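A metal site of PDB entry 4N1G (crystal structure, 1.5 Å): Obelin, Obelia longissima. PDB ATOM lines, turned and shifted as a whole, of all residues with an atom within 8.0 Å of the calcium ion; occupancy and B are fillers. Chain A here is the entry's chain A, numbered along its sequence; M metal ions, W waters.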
ATOM      1  N   PHE A 119     -35.272  28.343  18.150  1.00  0.00           N
ATOM      2  CA  PHE A 119     -34.774  27.971  16.839  1.00  0.00           C
ATOM      3  C   PHE A 119     -34.976  29.133  15.843  1.00  0.00           C
ATOM      4  O   PHE A 119     -34.029  29.539  15.106  1.00  0.00           O
ATOM      5  CB  PHE A 119     -35.495  26.731  16.339  1.00  0.00           C
ATOM      6  CG  PHE A 119     -34.966  26.232  15.064  1.00  0.00           C
ATOM      7  CD1 PHE A 119     -35.457  26.747  13.888  1.00  0.00           C
ATOM      8  CD2 PHE A 119     -33.909  25.300  15.045  1.00  0.00           C
ATOM      9  CE1 PHE A 119     -34.924  26.302  12.638  1.00  0.00           C
ATOM     10  CE2 PHE A 119     -33.376  24.869  13.850  1.00  0.00           C
ATOM     11  CZ  PHE A 119     -33.868  25.380  12.650  1.00  0.00           C
ATOM     12  N   PHE A 122     -32.336  31.726  16.440  1.00  0.00           N
ATOM     13  CA  PHE A 122     -31.014  31.338  15.990  1.00  0.00           C
ATOM     14  C   PHE A 122     -30.862  31.313  14.481  1.00  0.00           C
ATOM     15  O   PHE A 122     -29.771  31.496  13.956  1.00  0.00           O
ATOM     16  CB  PHE A 122     -30.706  29.933  16.483  1.00  0.00           C
ATOM     17  CG  PHE A 122     -30.328  29.804  17.945  1.00  0.00           C
ATOM     18  CD1 PHE A 122     -30.112  30.869  18.764  1.00  0.00           C
ATOM     19  CD2 PHE A 122     -30.074  28.553  18.464  1.00  0.00           C
ATOM     20  CE1 PHE A 122     -29.752  30.671  20.101  1.00  0.00           C
ATOM     21  CE2 PHE A 122     -29.708  28.371  19.790  1.00  0.00           C
ATOM     22  CZ  PHE A 122     -29.524  29.454  20.583  1.00  0.00           C
ATOM     23  N   ASP A 123     -31.961  30.982  13.800  1.00  0.00           N
ATOM     24  CA  ASP A 123     -31.942  30.789  12.345  1.00  0.00           C
ATOM     25  C   ASP A 123     -32.022  32.171  11.614  1.00  0.00           C
ATOM     26  O   ASP A 123     -33.063  32.554  11.030  1.00  0.00           O
ATOM     27  CB  ASP A 123     -33.061  29.834  11.911  1.00  0.00           C
ATOM     28  CG  ASP A 123     -32.976  29.493  10.427  1.00  0.00           C
ATOM     29  OD1 ASP A 123     -31.898  29.675   9.804  1.00  0.00           O
ATOM     30  OD2 ASP A 123     -34.030  29.093   9.888  1.00  0.00           O
ATOM     31  N   LYS A 124     -30.907  32.903  11.732  1.00  0.00           N
ATOM     32  CA  LYS A 124     -30.867  34.326  11.321  1.00  0.00           C
ATOM     33  C   LYS A 124     -31.098  34.468   9.846  1.00  0.00           C
ATOM     34  O   LYS A 124     -31.668  35.492   9.419  1.00  0.00           O
ATOM     35  CB  LYS A 124     -29.552  34.981  11.724  1.00  0.00           C
ATOM     36  CG  LYS A 124     -29.441  35.221  13.241  1.00  0.00           C
ATOM     37  CD  LYS A 124     -30.387  36.332  13.677  1.00  0.00           C
ATOM     38  CE  LYS A 124     -30.136  36.655  15.187  1.00  0.00           C
ATOM     39  NZ  LYS A 124     -30.971  37.847  15.580  1.00  0.00           N
ATOM     40  N   ASP A 125     -30.720  33.467   9.049  1.00  0.00           N
ATOM     41  CA  ASP A 125     -30.905  33.634   7.597  1.00  0.00           C
ATOM     42  C   ASP A 125     -32.208  32.982   7.115  1.00  0.00           C
ATOM     43  O   ASP A 125     -32.507  33.038   5.918  1.00  0.00           O
ATOM     44  CB  ASP A 125     -29.696  33.116   6.797  1.00  0.00           C
ATOM     45  CG  ASP A 125     -29.446  31.605   6.965  1.00  0.00           C
ATOM     46  OD1 ASP A 125     -30.246  30.919   7.637  1.00  0.00           O
ATOM     47  OD2 ASP A 125     -28.449  31.100   6.362  1.00  0.00           O
ATOM     48  N   GLY A 126     -32.985  32.408   8.012  1.00  0.00           N
ATOM     49  CA  GLY A 126     -34.268  31.805   7.698  1.00  0.00           C
ATOM     50  C   GLY A 126     -34.157  30.563   6.819  1.00  0.00           C
ATOM     51  O   GLY A 126     -35.121  30.197   6.122  1.00  0.00           O
ATOM     52  N   SER A 127     -33.027  29.876   6.877  1.00  0.00           N
ATOM     53  CA  SER A 127     -32.794  28.758   5.964  1.00  0.00           C
ATOM     54  C   SER A 127     -33.548  27.493   6.368  1.00  0.00           C
ATOM     55  O   SER A 127     -33.686  26.549   5.543  1.00  0.00           O
ATOM     56  CB  SER A 127     -31.314  28.468   5.880  1.00  0.00           C
ATOM     57  OG  SER A 127     -30.850  27.964   7.147  1.00  0.00           O
ATOM     58  N   GLY A 128     -33.961  27.413   7.629  1.00  0.00           N
ATOM     59  CA  GLY A 128     -34.655  26.268   8.197  1.00  0.00           C
ATOM     60  C   GLY A 128     -33.734  25.292   8.858  1.00  0.00           C
ATOM     61  O   GLY A 128     -34.138  24.219   9.373  1.00  0.00           O
ATOM     62  N   THR A 129     -32.442  25.642   8.873  1.00  0.00           N
ATOM     63  CA  THR A 129     -31.454  24.882   9.674  1.00  0.00           C
ATOM     64  C   THR A 129     -30.470  25.857  10.300  1.00  0.00           C
ATOM     65  O   THR A 129     -30.288  26.998   9.838  1.00  0.00           O
ATOM     66  CB  THR A 129     -30.656  23.795   8.868  1.00  0.00           C
ATOM     67  OG1 THR A 129     -29.911  24.403   7.821  1.00  0.00           O
ATOM     68  CG2 THR A 129     -31.568  22.721   8.283  1.00  0.00           C
ATOM     69  N   ILE A 130     -29.810  25.396  11.369  1.00  0.00           N
ATOM     70  CA  ILE A 130     -28.818  26.147  12.118  1.00  0.00           C
ATOM     71  C   ILE A 130     -27.441  25.661  11.649  1.00  0.00           C
ATOM     72  O   ILE A 130     -27.087  24.463  11.807  1.00  0.00           O
ATOM     73  CB  ILE A 130     -28.988  25.979  13.689  1.00  0.00           C
ATOM     74  CG1 ILE A 130     -30.423  26.288  14.111  1.00  0.00           C
ATOM     75  CG2 ILE A 130     -27.968  26.819  14.468  1.00  0.00           C
ATOM     76  CD1 ILE A 130     -30.941  27.623  13.590  1.00  0.00           C
ATOM     77  N   THR A 131     -26.671  26.544  11.057  1.00  0.00           N
ATOM     78  CA  THR A 131     -25.313  26.205  10.660  1.00  0.00           C
ATOM     79  C   THR A 131     -24.319  26.579  11.781  1.00  0.00           C
ATOM     80  O   THR A 131     -24.729  27.314  12.710  1.00  0.00           O
ATOM     81  CB  THR A 131     -24.954  26.880   9.326  1.00  0.00           C
ATOM     82  OG1 THR A 131     -25.349  28.247   9.348  1.00  0.00           O
ATOM     83  CG2 THR A 131     -25.773  26.172   8.222  1.00  0.00           C
ATOM     84  N   LEU A 132     -23.090  26.081  11.688  1.00  0.00           N
ATOM     85  CA  LEU A 132     -22.165  26.268  12.834  1.00  0.00           C
ATOM     86  C   LEU A 132     -21.983  27.797  13.116  1.00  0.00           C
ATOM     87  O   LEU A 132     -21.898  28.226  14.289  1.00  0.00           O
ATOM     88  CB  LEU A 132     -20.842  25.575  12.587  1.00  0.00           C
ATOM     89  CG  LEU A 132     -19.764  25.644  13.684  1.00  0.00           C
ATOM     90  CD1 LEU A 132     -20.187  24.974  14.991  1.00  0.00           C
ATOM     91  CD2 LEU A 132     -18.473  25.128  13.181  1.00  0.00           C
ATOM     92  N   ASP A 133     -21.963  28.612  12.072  1.00  0.00           N
ATOM     93  CA  ASP A 133     -21.782  30.081  12.268  1.00  0.00           C
ATOM     94  C   ASP A 133     -22.960  30.737  13.045  1.00  0.00           C
ATOM     95  O   ASP A 133     -22.773  31.791  13.673  1.00  0.00           O
ATOM     96  CB  ASP A 133     -21.599  30.769  10.914  1.00  0.00           C
ATOM     97  CG  ASP A 133     -22.852  30.607  10.010  1.00  0.00           C
ATOM     98  OD1 ASP A 133     -23.135  29.451   9.623  1.00  0.00           O
ATOM     99  OD2 ASP A 133     -23.547  31.618   9.698  1.00  0.00           O
ATOM    100  N   GLU A 134     -24.155  30.151  13.019  1.00  0.00           N
ATOM    101  CA  GLU A 134     -25.316  30.641  13.752  1.00  0.00           C
ATOM    102  C   GLU A 134     -25.338  30.127  15.219  1.00  0.00           C
ATOM    103  O   GLU A 134     -26.097  30.589  16.050  1.00  0.00           O
ATOM    104  CB  GLU A 134     -26.566  30.178  13.020  1.00  0.00           C
ATOM    105  CG  GLU A 134     -26.814  31.005  11.762  1.00  0.00           C
ATOM    106  CD  GLU A 134     -27.930  30.435  10.898  1.00  0.00           C
ATOM    107  OE1 GLU A 134     -28.231  29.182  10.924  1.00  0.00           O
ATOM    108  OE2 GLU A 134     -28.618  31.213  10.189  1.00  0.00           O
ATOM    109  N   ASP A 165     -25.654  20.380  10.036  1.00  0.00           N
ATOM    110  CA  ASP A 165     -26.491  21.492  10.497  1.00  0.00           C
ATOM    111  C   ASP A 165     -27.574  20.980  11.410  1.00  0.00           C
ATOM    112  O   ASP A 165     -27.751  19.719  11.527  1.00  0.00           O
ATOM    113  CB  ASP A 165     -27.094  22.300   9.332  1.00  0.00           C
ATOM    114  CG  ASP A 165     -27.873  21.472   8.316  1.00  0.00           C
ATOM    115  OD1 ASP A 165     -28.202  20.267   8.523  1.00  0.00           O
ATOM    116  OD2 ASP A 165     -28.168  22.056   7.233  1.00  0.00           O
ATOM    117  N   LEU A 166     -28.244  21.892  12.110  1.00  0.00           N
ATOM    118  CA  LEU A 166     -29.231  21.479  13.123  1.00  0.00           C
ATOM    119  C   LEU A 166     -30.642  21.808  12.684  1.00  0.00           C
ATOM    120  O   LEU A 166     -30.922  22.918  12.152  1.00  0.00           O
ATOM    121  CB  LEU A 166     -28.996  22.159  14.476  1.00  0.00           C
ATOM    122  CG  LEU A 166     -27.548  22.078  14.923  1.00  0.00           C
ATOM    123  CD1 LEU A 166     -27.449  22.857  16.253  1.00  0.00           C
ATOM    124  CD2 LEU A 166     -27.138  20.629  15.136  1.00  0.00           C
HETATM  125 CA    CA M   1     -29.823  29.136   9.085  1.00  0.00          CA
HETATM  126  O   HOH W   1     -27.705  28.906   7.903  1.00  0.00           O
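OD1 of Asp 123 lies close to N of Gly 126 (3.4 Å). N of Gly 128 is in hydrogen-bond range of OD2 of Asp 123 (2.8 Å). OG1 of Thr 129 is in hydrogen-bond range of OD2 of Asp 165, at 3.0 Å. The side-chain carboxylate of Glu 134 lies close to the backbone NH of Thr 131 (3.1 Å). N of Lys 124 lies close to OE2 of Glu 134, at 3.2 Å.
Five residues have an atom within 4 Å of the calcium ion: Asp 123, Asp 125, Ser 127, Thr 129 and Glu 134. Along chain A the residues within 4 Å of the calcium ion span positions 123 to 134. The nearest printed residue that does not touch the calcium ion is Ile 130 (4.4 Å).
The calcium ion is bound by the side-chain carboxylate (OD1) of Asp 123, the backbone carbonyl oxygen (O) of Thr 129, the side-chain carboxylate (OD1) of Asp 125, the side-chain carboxylate (OE1) of Glu 134, water W1, the side-chain hydroxyl (OG) of Ser 127 and the side-chain carboxylate (OE2) of Glu 134. The calcium ion has seven donor atoms within binding distance.
Water W1 lies within hydrogen-bond range of the side-chain carboxylate of Asp 125 (2.8 Å) and the side-chain hydroxyl of Thr 131 (2.8 Å).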
